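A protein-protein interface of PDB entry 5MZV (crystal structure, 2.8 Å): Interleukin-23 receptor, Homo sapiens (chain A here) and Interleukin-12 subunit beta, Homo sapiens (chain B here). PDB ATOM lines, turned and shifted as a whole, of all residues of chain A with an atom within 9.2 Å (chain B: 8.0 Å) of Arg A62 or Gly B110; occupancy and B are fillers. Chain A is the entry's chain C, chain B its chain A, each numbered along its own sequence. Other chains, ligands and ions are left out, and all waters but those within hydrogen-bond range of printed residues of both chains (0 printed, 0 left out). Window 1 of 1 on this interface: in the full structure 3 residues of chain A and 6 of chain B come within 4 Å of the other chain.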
ATOM      1  N   ALA A  54       6.837   6.421  10.283  1.00  0.00           N
ATOM      2  CA  ALA A  54       6.365   5.488   9.274  1.00  0.00           C
ATOM      3  C   ALA A  54       5.937   6.232   8.018  1.00  0.00           C
ATOM      4  O   ALA A  54       5.504   7.387   8.069  1.00  0.00           O
ATOM      5  CB  ALA A  54       5.196   4.663   9.809  1.00  0.00           C
ATOM      6  N   ILE A  56       4.160   4.221   5.226  1.00  0.00           N
ATOM      7  CA  ILE A  56       3.496   3.193   4.432  1.00  0.00           C
ATOM      8  C   ILE A  56       2.396   3.854   3.613  1.00  0.00           C
ATOM      9  O   ILE A  56       1.621   4.665   4.135  1.00  0.00           O
ATOM     10  CB  ILE A  56       2.915   2.089   5.331  1.00  0.00           C
ATOM     11  CG1 ILE A  56       3.914   1.642   6.404  1.00  0.00           C
ATOM     12  CG2 ILE A  56       2.480   0.896   4.480  1.00  0.00           C
ATOM     13  CD1 ILE A  56       5.157   1.017   5.861  1.00  0.00           C
ATOM     14  N   CYS A  59      -1.829   3.283   4.840  1.00  0.00           N
ATOM     15  CA  CYS A  59      -1.831   2.708   6.179  1.00  0.00           C
ATOM     16  C   CYS A  59      -1.525   3.765   7.231  1.00  0.00           C
ATOM     17  O   CYS A  59      -0.413   4.299   7.279  1.00  0.00           O
ATOM     18  CB  CYS A  59      -0.818   1.562   6.286  1.00  0.00           C
ATOM     19  SG  CYS A  59      -0.386   1.144   8.008  1.00  0.00           S
ATOM     20  N   GLN A  60      -2.516   4.081   8.067  1.00  0.00           N
ATOM     21  CA  GLN A  60      -2.272   4.825   9.294  1.00  0.00           C
ATOM     22  C   GLN A  60      -1.905   3.810  10.368  1.00  0.00           C
ATOM     23  O   GLN A  60      -2.783   3.053  10.809  1.00  0.00           O
ATOM     24  CB  GLN A  60      -3.502   5.621   9.707  1.00  0.00           C
ATOM     25  CG  GLN A  60      -3.920   6.684   8.701  1.00  0.00           C
ATOM     26  CD  GLN A  60      -2.803   7.665   8.383  1.00  0.00           C
ATOM     27  OE1 GLN A  60      -2.536   8.593   9.150  1.00  0.00           O
ATOM     28  NE2 GLN A  60      -2.142   7.460   7.249  1.00  0.00           N
ATOM     29  N   PRO A  61      -0.647   3.729  10.797  1.00  0.00           N
ATOM     30  CA  PRO A  61      -0.262   2.670  11.737  1.00  0.00           C
ATOM     31  C   PRO A  61      -1.135   2.667  12.983  1.00  0.00           C
ATOM     32  O   PRO A  61      -1.317   3.693  13.642  1.00  0.00           O
ATOM     33  CB  PRO A  61       1.196   3.004  12.066  1.00  0.00           C
ATOM     34  CG  PRO A  61       1.678   3.795  10.903  1.00  0.00           C
ATOM     35  CD  PRO A  61       0.496   4.584  10.435  1.00  0.00           C
ATOM     36  N   ARG A  62      -1.690   1.494  13.295  1.00  0.00           N
ATOM     37  CA  ARG A  62      -2.438   1.328  14.537  1.00  0.00           C
ATOM     38  C   ARG A  62      -1.515   1.460  15.742  1.00  0.00           C
ATOM     39  O   ARG A  62      -1.838   2.155  16.712  1.00  0.00           O
ATOM     40  CB  ARG A  62      -3.139  -0.029  14.537  1.00  0.00           C
ATOM     41  CG  ARG A  62      -3.966  -0.313  15.774  1.00  0.00           C
ATOM     42  CD  ARG A  62      -4.455  -1.751  15.788  1.00  0.00           C
ATOM     43  NE  ARG A  62      -5.299  -2.024  16.950  1.00  0.00           N
ATOM     44  CZ  ARG A  62      -4.846  -2.395  18.144  1.00  0.00           C
ATOM     45  NH1 ARG A  62      -3.544  -2.547  18.356  1.00  0.00           N
ATOM     46  NH2 ARG A  62      -5.701  -2.615  19.135  1.00  0.00           N
ATOM     47  N   LYS A  63      -0.364   0.792  15.696  1.00  0.00           N
ATOM     48  CA  LYS A  63       0.675   0.943  16.701  1.00  0.00           C
ATOM     49  C   LYS A  63       2.030   0.962  16.012  1.00  0.00           C
ATOM     50  O   LYS A  63       2.191   0.465  14.895  1.00  0.00           O
ATOM     51  CB  LYS A  63       0.649  -0.186  17.740  1.00  0.00           C
ATOM     52  CG  LYS A  63      -0.354   0.011  18.861  1.00  0.00           C
ATOM     53  CD  LYS A  63       0.124  -0.644  20.151  1.00  0.00           C
ATOM     54  CE  LYS A  63       1.242   0.160  20.812  1.00  0.00           C
ATOM     55  NZ  LYS A  63       1.655  -0.431  22.122  1.00  0.00           N
ATOM     56  N   LEU A  64       3.010   1.543  16.701  1.00  0.00           N
ATOM     57  CA  LEU A  64       4.392   1.577  16.240  1.00  0.00           C
ATOM     58  C   LEU A  64       5.256   0.888  17.283  1.00  0.00           C
ATOM     59  O   LEU A  64       5.307   1.327  18.437  1.00  0.00           O
ATOM     60  CB  LEU A  64       4.856   3.015  16.008  1.00  0.00           C
ATOM     61  CG  LEU A  64       4.263   3.699  14.775  1.00  0.00           C
ATOM     62  CD1 LEU A  64       4.470   5.200  14.847  1.00  0.00           C
ATOM     63  CD2 LEU A  64       4.886   3.141  13.513  1.00  0.00           C
ATOM     64  N   HIS A  65       5.928  -0.185  16.878  1.00  0.00           N
ATOM     65  CA  HIS A  65       6.718  -1.004  17.783  1.00  0.00           C
ATOM     66  C   HIS A  65       8.203  -0.770  17.560  1.00  0.00           C
ATOM     67  O   HIS A  65       8.643  -0.494  16.444  1.00  0.00           O
ATOM     68  CB  HIS A  65       6.416  -2.491  17.587  1.00  0.00           C
ATOM     69  CG  HIS A  65       5.003  -2.867  17.896  1.00  0.00           C
ATOM     70  ND1 HIS A  65       4.410  -2.598  19.110  1.00  0.00           N
ATOM     71  CD2 HIS A  65       4.067  -3.501  17.151  1.00  0.00           C
ATOM     72  CE1 HIS A  65       3.166  -3.044  19.097  1.00  0.00           C
ATOM     73  NE2 HIS A  65       2.935  -3.597  17.920  1.00  0.00           N
ATOM     74  N   ARG A  79       3.328   7.541  21.576  1.00  0.00           N
ATOM     75  CA  ARG A  79       2.898   7.827  20.213  1.00  0.00           C
ATOM     76  C   ARG A  79       2.775   9.336  20.052  1.00  0.00           C
ATOM     77  O   ARG A  79       1.843   9.950  20.583  1.00  0.00           O
ATOM     78  CB  ARG A  79       1.573   7.132  19.914  1.00  0.00           C
ATOM     79  CG  ARG A  79       1.035   7.377  18.510  1.00  0.00           C
ATOM     80  CD  ARG A  79       1.939   6.780  17.444  1.00  0.00           C
ATOM     81  NE  ARG A  79       1.279   6.729  16.141  1.00  0.00           N
ATOM     82  CZ  ARG A  79       0.475   5.745  15.744  1.00  0.00           C
ATOM     83  NH1 ARG A  79       0.221   4.715  16.543  1.00  0.00           N
ATOM     84  NH2 ARG A  79      -0.081   5.788  14.540  1.00  0.00           N
ATOM     85  N   ASN A  81       2.541  11.462  17.050  1.00  0.00           N
ATOM     86  CA  ASN A  81       1.423  11.799  16.181  1.00  0.00           C
ATOM     87  C   ASN A  81       1.131  10.606  15.274  1.00  0.00           C
ATOM     88  O   ASN A  81       1.703   9.521  15.429  1.00  0.00           O
ATOM     89  CB  ASN A  81       1.699  13.098  15.407  1.00  0.00           C
ATOM     90  CG  ASN A  81       3.015  13.078  14.648  1.00  0.00           C
ATOM     91  OD1 ASN A  81       3.413  12.056  14.086  1.00  0.00           O
ATOM     92  ND2 ASN A  81       3.698  14.228  14.627  1.00  0.00           N
ATOM     93  N   LYS A  82       0.223  10.820  14.320  1.00  0.00           N
ATOM     94  CA  LYS A  82      -0.367   9.722  13.559  1.00  0.00           C
ATOM     95  C   LYS A  82       0.674   8.821  12.913  1.00  0.00           C
ATOM     96  O   LYS A  82       0.372   7.660  12.617  1.00  0.00           O
ATOM     97  CB  LYS A  82      -1.298  10.271  12.469  1.00  0.00           C
ATOM     98  CG  LYS A  82      -2.196  11.421  12.922  1.00  0.00           C
ATOM     99  CD  LYS A  82      -1.548  12.780  12.656  1.00  0.00           C
ATOM    100  CE  LYS A  82      -1.766  13.744  13.816  1.00  0.00           C
ATOM    101  NZ  LYS A  82      -0.943  14.980  13.669  1.00  0.00           N
ATOM    102  N   THR A  83       1.888   9.320  12.681  1.00  0.00           N
ATOM    103  CA  THR A  83       2.894   8.563  11.953  1.00  0.00           C
ATOM    104  C   THR A  83       4.212   8.394  12.695  1.00  0.00           C
ATOM    105  O   THR A  83       5.078   7.662  12.201  1.00  0.00           O
ATOM    106  CB  THR A  83       3.175   9.229  10.594  1.00  0.00           C
ATOM    107  OG1 THR A  83       4.265   8.563   9.940  1.00  0.00           O
ATOM    108  CG2 THR A  83       3.500  10.711  10.773  1.00  0.00           C
ATOM    109  N   ALA A  85       6.501   7.775  16.430  1.00  0.00           N
ATOM    110  CA  ALA A  85       6.560   7.293  17.800  1.00  0.00           C
ATOM    111  C   ALA A  85       7.950   7.558  18.359  1.00  0.00           C
ATOM    112  O   ALA A  85       8.922   7.697  17.613  1.00  0.00           O
ATOM    113  CB  ALA A  85       6.229   5.796  17.890  1.00  0.00           C
ATOM    114  N   THR A 102       8.546  -1.191  13.652  1.00  0.00           N
ATOM    115  CA  THR A 102       7.556  -1.766  12.757  1.00  0.00           C
ATOM    116  C   THR A 102       6.233  -1.038  12.936  1.00  0.00           C
ATOM    117  O   THR A 102       6.073  -0.196  13.824  1.00  0.00           O
ATOM    118  CB  THR A 102       7.372  -3.264  13.023  1.00  0.00           C
ATOM    119  OG1 THR A 102       6.746  -3.451  14.298  1.00  0.00           O
ATOM    120  CG2 THR A 102       8.712  -3.978  13.023  1.00  0.00           C
ATOM    121  N   ALA A 103       5.279  -1.380  12.077  1.00  0.00           N
ATOM    122  CA  ALA A 103       3.947  -0.795  12.109  1.00  0.00           C
ATOM    123  C   ALA A 103       2.897  -1.893  12.051  1.00  0.00           C
ATOM    124  O   ALA A 103       3.056  -2.883  11.330  1.00  0.00           O
ATOM    125  CB  ALA A 103       3.741   0.179  10.944  1.00  0.00           C
ATOM    126  N   GLU A 104       1.830  -1.716  12.823  1.00  0.00           N
ATOM    127  CA  GLU A 104       0.648  -2.562  12.725  1.00  0.00           C
ATOM    128  C   GLU A 104      -0.321  -1.905  11.752  1.00  0.00           C
ATOM    129  O   GLU A 104      -0.945  -0.889  12.079  1.00  0.00           O
ATOM    130  CB  GLU A 104      -0.001  -2.760  14.093  1.00  0.00           C
ATOM    131  CG  GLU A 104       0.753  -3.699  15.022  1.00  0.00           C
ATOM    132  CD  GLU A 104       0.025  -3.940  16.336  1.00  0.00           C
ATOM    133  OE1 GLU A 104      -1.162  -3.559  16.449  1.00  0.00           O
ATOM    134  OE2 GLU A 104       0.642  -4.511  17.260  1.00  0.00           O
ATOM    135  N   CYS A 105      -0.438  -2.471  10.548  1.00  0.00           N
ATOM    136  CA  CYS A 105      -1.367  -1.974   9.540  1.00  0.00           C
ATOM    137  C   CYS A 105      -2.670  -2.765   9.591  1.00  0.00           C
ATOM    138  O   CYS A 105      -2.628  -3.998   9.669  1.00  0.00           O
ATOM    139  CB  CYS A 105      -0.763  -2.106   8.143  1.00  0.00           C
ATOM    140  SG  CYS A 105       1.044  -1.926   8.088  1.00  0.00           S
ATOM    141  N   PRO A 106      -3.844  -2.126   9.540  1.00  0.00           N
ATOM    142  CA  PRO A 106      -5.094  -2.904   9.574  1.00  0.00           C
ATOM    143  C   PRO A 106      -5.210  -3.973   8.497  1.00  0.00           C
ATOM    144  O   PRO A 106      -5.868  -4.994   8.732  1.00  0.00           O
ATOM    145  CB  PRO A 106      -6.171  -1.826   9.408  1.00  0.00           C
ATOM    146  CG  PRO A 106      -5.576  -0.626  10.022  1.00  0.00           C
ATOM    147  CD  PRO A 106      -4.105  -0.683   9.703  1.00  0.00           C
ATOM    148  N   LYS A 107      -4.613  -3.782   7.323  1.00  0.00           N
ATOM    149  CA  LYS A 107      -4.799  -4.719   6.222  1.00  0.00           C
ATOM    150  C   LYS A 107      -3.766  -5.838   6.202  1.00  0.00           C
ATOM    151  O   LYS A 107      -3.682  -6.563   5.206  1.00  0.00           O
ATOM    152  CB  LYS A 107      -4.780  -3.979   4.880  1.00  0.00           C
ATOM    153  CG  LYS A 107      -3.493  -3.231   4.575  1.00  0.00           C
ATOM    154  CD  LYS A 107      -3.441  -2.812   3.109  1.00  0.00           C
ATOM    155  CE  LYS A 107      -3.064  -3.990   2.216  1.00  0.00           C
ATOM    156  NZ  LYS A 107      -3.830  -4.021   0.937  1.00  0.00           N
ATOM    157  N   HIS A 108      -2.987  -6.005   7.268  1.00  0.00           N
ATOM    158  CA  HIS A 108      -2.020  -7.090   7.349  1.00  0.00           C
ATOM    159  C   HIS A 108      -2.013  -7.660   8.757  1.00  0.00           C
ATOM    160  O   HIS A 108      -2.184  -6.928   9.735  1.00  0.00           O
ATOM    161  CB  HIS A 108      -0.604  -6.626   6.989  1.00  0.00           C
ATOM    162  CG  HIS A 108      -0.478  -6.073   5.606  1.00  0.00           C
ATOM    163  ND1 HIS A 108      -0.199  -4.746   5.361  1.00  0.00           N
ATOM    164  CD2 HIS A 108      -0.585  -6.666   4.394  1.00  0.00           C
ATOM    165  CE1 HIS A 108      -0.140  -4.545   4.056  1.00  0.00           C
ATOM    166  NE2 HIS A 108      -0.371  -5.694   3.447  1.00  0.00           N
ATOM    167  N   PHE A 109      -1.817  -8.973   8.853  1.00  0.00           N
ATOM    168  CA  PHE A 109      -1.639  -9.627  10.141  1.00  0.00           C
ATOM    169  C   PHE A 109      -0.189  -9.624  10.596  1.00  0.00           C
ATOM    170  O   PHE A 109       0.087  -9.986  11.744  1.00  0.00           O
ATOM    171  CB  PHE A 109      -2.159 -11.069  10.078  1.00  0.00           C
ATOM    172  CG  PHE A 109      -3.651 -11.170   9.908  1.00  0.00           C
ATOM    173  CD1 PHE A 109      -4.503 -10.343  10.621  1.00  0.00           C
ATOM    174  CD2 PHE A 109      -4.201 -12.093   9.034  1.00  0.00           C
ATOM    175  CE1 PHE A 109      -5.871 -10.434  10.467  1.00  0.00           C
ATOM    176  CE2 PHE A 109      -5.570 -12.188   8.876  1.00  0.00           C
ATOM    177  CZ  PHE A 109      -6.405 -11.358   9.593  1.00  0.00           C
ATOM    178  N   GLU A 111       3.525  -7.415  11.125  1.00  0.00           N
ATOM    179  CA  GLU A 111       4.059  -6.078  11.328  1.00  0.00           C
ATOM    180  C   GLU A 111       4.925  -5.705  10.132  1.00  0.00           C
ATOM    181  O   GLU A 111       5.785  -6.484   9.709  1.00  0.00           O
ATOM    182  CB  GLU A 111       4.863  -6.015  12.624  1.00  0.00           C
ATOM    183  CG  GLU A 111       4.047  -6.340  13.861  1.00  0.00           C
ATOM    184  CD  GLU A 111       4.860  -6.262  15.141  1.00  0.00           C
ATOM    185  OE1 GLU A 111       6.091  -6.055  15.057  1.00  0.00           O
ATOM    186  OE2 GLU A 111       4.270  -6.409  16.232  1.00  0.00           O
ATOM    187  N   ILE A 114       9.468  -0.820   9.150  1.00  0.00           N
ATOM    188  CA  ILE A 114       9.613   0.589   8.805  1.00  0.00           C
ATOM    189  C   ILE A 114      11.061   0.842   8.413  1.00  0.00           C
ATOM    190  O   ILE A 114      11.359   1.097   7.242  1.00  0.00           O
ATOM    191  CB  ILE A 114       9.172   1.495   9.967  1.00  0.00           C
ATOM    192  CG1 ILE A 114       7.650   1.444  10.101  1.00  0.00           C
ATOM    193  CG2 ILE A 114       9.638   2.930   9.749  1.00  0.00           C
ATOM    194  CD1 ILE A 114       7.140   2.047  11.376  1.00  0.00           C
ATOM    195  N   ASP B  36     -15.320   3.284  10.966  1.00  0.00           N
ATOM    196  CA  ASP B  36     -14.479   3.165  12.154  1.00  0.00           C
ATOM    197  C   ASP B  36     -15.370   3.453  13.354  1.00  0.00           C
ATOM    198  O   ASP B  36     -15.606   4.612  13.701  1.00  0.00           O
ATOM    199  CB  ASP B  36     -13.299   4.126  12.082  1.00  0.00           C
ATOM    200  CG  ASP B  36     -12.526   4.194  13.383  1.00  0.00           C
ATOM    201  OD1 ASP B  36     -12.018   3.143  13.835  1.00  0.00           O
ATOM    202  OD2 ASP B  36     -12.428   5.300  13.954  1.00  0.00           O
ATOM    203  N   TRP B  37     -15.884   2.400  13.985  1.00  0.00           N
ATOM    204  CA  TRP B  37     -16.894   2.572  15.016  1.00  0.00           C
ATOM    205  C   TRP B  37     -16.282   2.643  16.405  1.00  0.00           C
ATOM    206  O   TRP B  37     -15.403   1.854  16.761  1.00  0.00           O
ATOM    207  CB  TRP B  37     -17.931   1.450  14.998  1.00  0.00           C
ATOM    208  CG  TRP B  37     -19.008   1.748  15.987  1.00  0.00           C
ATOM    209  CD1 TRP B  37     -20.088   2.556  15.794  1.00  0.00           C
ATOM    210  CD2 TRP B  37     -19.087   1.287  17.339  1.00  0.00           C
ATOM    211  NE1 TRP B  37     -20.839   2.620  16.938  1.00  0.00           N
ATOM    212  CE2 TRP B  37     -20.247   1.848  17.903  1.00  0.00           C
ATOM    213  CE3 TRP B  37     -18.290   0.452  18.128  1.00  0.00           C
ATOM    214  CZ2 TRP B  37     -20.634   1.595  19.217  1.00  0.00           C
ATOM    215  CZ3 TRP B  37     -18.677   0.204  19.432  1.00  0.00           C
ATOM    216  CH2 TRP B  37     -19.836   0.773  19.963  1.00  0.00           C
ATOM    217  N   LYS B 106     -16.834  -2.985   8.945  1.00  0.00           N
ATOM    218  CA  LYS B 106     -16.703  -2.419  10.278  1.00  0.00           C
ATOM    219  C   LYS B 106     -15.266  -2.543  10.757  1.00  0.00           C
ATOM    220  O   LYS B 106     -14.687  -3.633  10.748  1.00  0.00           O
ATOM    221  CB  LYS B 106     -17.652  -3.117  11.252  1.00  0.00           C
ATOM    222  CG  LYS B 106     -17.847  -2.369  12.555  1.00  0.00           C
ATOM    223  CD  LYS B 106     -18.803  -3.108  13.489  1.00  0.00           C
ATOM    224  CE  LYS B 106     -18.095  -4.199  14.286  1.00  0.00           C
ATOM    225  NZ  LYS B 106     -17.072  -3.627  15.214  1.00  0.00           N
ATOM    226  N   LYS B 107     -14.698  -1.418  11.168  1.00  0.00           N
ATOM    227  CA  LYS B 107     -13.379  -1.355  11.779  1.00  0.00           C
ATOM    228  C   LYS B 107     -13.560  -0.824  13.190  1.00  0.00           C
ATOM    229  O   LYS B 107     -14.255   0.177  13.393  1.00  0.00           O
ATOM    230  CB  LYS B 107     -12.452  -0.452  10.955  1.00  0.00           C
ATOM    231  CG  LYS B 107     -11.074  -0.214  11.546  1.00  0.00           C
ATOM    232  CD  LYS B 107     -10.125   0.397  10.511  1.00  0.00           C
ATOM    233  CE  LYS B 107     -10.612   1.747  10.007  1.00  0.00           C
ATOM    234  NZ  LYS B 107      -9.668   2.346   9.021  1.00  0.00           N
ATOM    235  N   GLU B 108     -12.975  -1.506  14.168  1.00  0.00           N
ATOM    236  CA  GLU B 108     -13.095  -1.103  15.564  1.00  0.00           C
ATOM    237  C   GLU B 108     -11.710  -1.120  16.191  1.00  0.00           C
ATOM    238  O   GLU B 108     -11.086  -2.181  16.296  1.00  0.00           O
ATOM    239  CB  GLU B 108     -14.054  -2.020  16.328  1.00  0.00           C
ATOM    240  CG  GLU B 108     -14.431  -1.503  17.709  1.00  0.00           C
ATOM    241  CD  GLU B 108     -15.533  -2.322  18.366  1.00  0.00           C
ATOM    242  OE1 GLU B 108     -16.067  -3.249  17.715  1.00  0.00           O
ATOM    243  OE2 GLU B 108     -15.865  -2.038  19.536  1.00  0.00           O
ATOM    244  N   ASP B 109     -11.231   0.056  16.593  1.00  0.00           N
ATOM    245  CA  ASP B 109      -9.917   0.197  17.216  1.00  0.00           C
ATOM    246  C   ASP B 109      -8.817  -0.312  16.286  1.00  0.00           C
ATOM    247  O   ASP B 109      -7.862  -0.960  16.715  1.00  0.00           O
ATOM    248  CB  ASP B 109      -9.872  -0.521  18.566  1.00  0.00           C
ATOM    249  CG  ASP B 109      -8.644  -0.154  19.380  1.00  0.00           C
ATOM    250  OD1 ASP B 109      -8.425   1.054  19.622  1.00  0.00           O
ATOM    251  OD2 ASP B 109      -7.899  -1.073  19.783  1.00  0.00           O
ATOM    252  N   GLY B 110      -8.957  -0.017  14.996  1.00  0.00           N
ATOM    253  CA  GLY B 110      -7.930  -0.351  14.031  1.00  0.00           C
ATOM    254  C   GLY B 110      -7.917  -1.784  13.554  1.00  0.00           C
ATOM    255  O   GLY B 110      -6.908  -2.225  12.999  1.00  0.00           O
ATOM    256  N   ILE B 111      -9.004  -2.528  13.741  1.00  0.00           N
ATOM    257  CA  ILE B 111      -9.062  -3.941  13.383  1.00  0.00           C
ATOM    258  C   ILE B 111     -10.336  -4.177  12.587  1.00  0.00           C
ATOM    259  O   ILE B 111     -11.436  -3.916  13.085  1.00  0.00           O
ATOM    260  CB  ILE B 111      -9.032  -4.848  14.624  1.00  0.00           C
ATOM    261  CG1 ILE B 111      -7.827  -4.524  15.511  1.00  0.00           C
ATOM    262  CG2 ILE B 111      -8.985  -6.315  14.210  1.00  0.00           C
ATOM    263  CD1 ILE B 111      -8.047  -4.867  16.964  1.00  0.00           C
ATOM    264  N   TRP B 112     -10.192  -4.671  11.357  1.00  0.00           N
ATOM    265  CA  TRP B 112     -11.356  -5.045  10.566  1.00  0.00           C
ATOM    266  C   TRP B 112     -12.049  -6.243  11.200  1.00  0.00           C
ATOM    267  O   TRP B 112     -11.396  -7.141  11.738  1.00  0.00           O
ATOM    268  CB  TRP B 112     -10.957  -5.396   9.132  1.00  0.00           C
ATOM    269  CG  TRP B 112     -10.360  -4.282   8.342  1.00  0.00           C
ATOM    270  CD1 TRP B 112      -9.069  -4.183   7.922  1.00  0.00           C
ATOM    271  CD2 TRP B 112     -11.029  -3.112   7.860  1.00  0.00           C
ATOM    272  NE1 TRP B 112      -8.888  -3.024   7.213  1.00  0.00           N
ATOM    273  CE2 TRP B 112     -10.077  -2.346   7.162  1.00  0.00           C
ATOM    274  CE3 TRP B 112     -12.338  -2.637   7.956  1.00  0.00           C
ATOM    275  CZ2 TRP B 112     -10.392  -1.129   6.560  1.00  0.00           C
ATOM    276  CZ3 TRP B 112     -12.649  -1.423   7.360  1.00  0.00           C
ATOM    277  CH2 TRP B 112     -11.679  -0.686   6.671  1.00  0.00           C
ATOM    278  N   SER B 113     -13.379  -6.261  11.125  1.00  0.00           N
ATOM    279  CA  SER B 113     -14.138  -7.368  11.689  1.00  0.00           C
ATOM    280  C   SER B 113     -13.827  -8.665  10.951  1.00  0.00           C
ATOM    281  O   SER B 113     -13.518  -8.672   9.756  1.00  0.00           O
ATOM    282  CB  SER B 113     -15.639  -7.079  11.625  1.00  0.00           C
ATOM    283  OG  SER B 113     -16.109  -7.065  10.286  1.00  0.00           O
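The side-chain carboxylate (OD2) of Asp B109 lies within salt-bridge range of the guanidinium group (NH2) of Arg A62, at 2.8 Å.
The guanidinium group of Arg A79 sits at hydrogen-bond distance from the backbone carbonyl oxygen of Arg A62 (3.3 Å).
NH1 of Arg A62 is in salt-bridge range of OE1 of Glu A104, 3.2 Å away.
Among the printed residues, merely in contact across the chains: Pro A106 with Trp B112 (3.4 Å), Pro A106 with Gly B110 (3.6 Å), Arg A62 with Gly B110 (3.7 Å) and Arg A62 with Ile B111 (3.8 Å).
Arg A62 touches just these residues of chain B: Asp B109, Gly B110 and Ile B111.
Arg A79 touches none of the printed residues of chain B.
Of the printed residues of chain B, Pro A106 touches Gly B110 and Trp B112.
Lys A107 touches none of the printed residues of chain B.
Asp B109 touches one residue of chain A.
Of chain A, only Arg A62 (3.8 Å) comes within 4 Å of Ile B111.
Printed residues of chain A within 4 Å of Trp B112: Pro A106 (3.4 Å).
Among the printed residues, 5 pairs touch across the chains.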
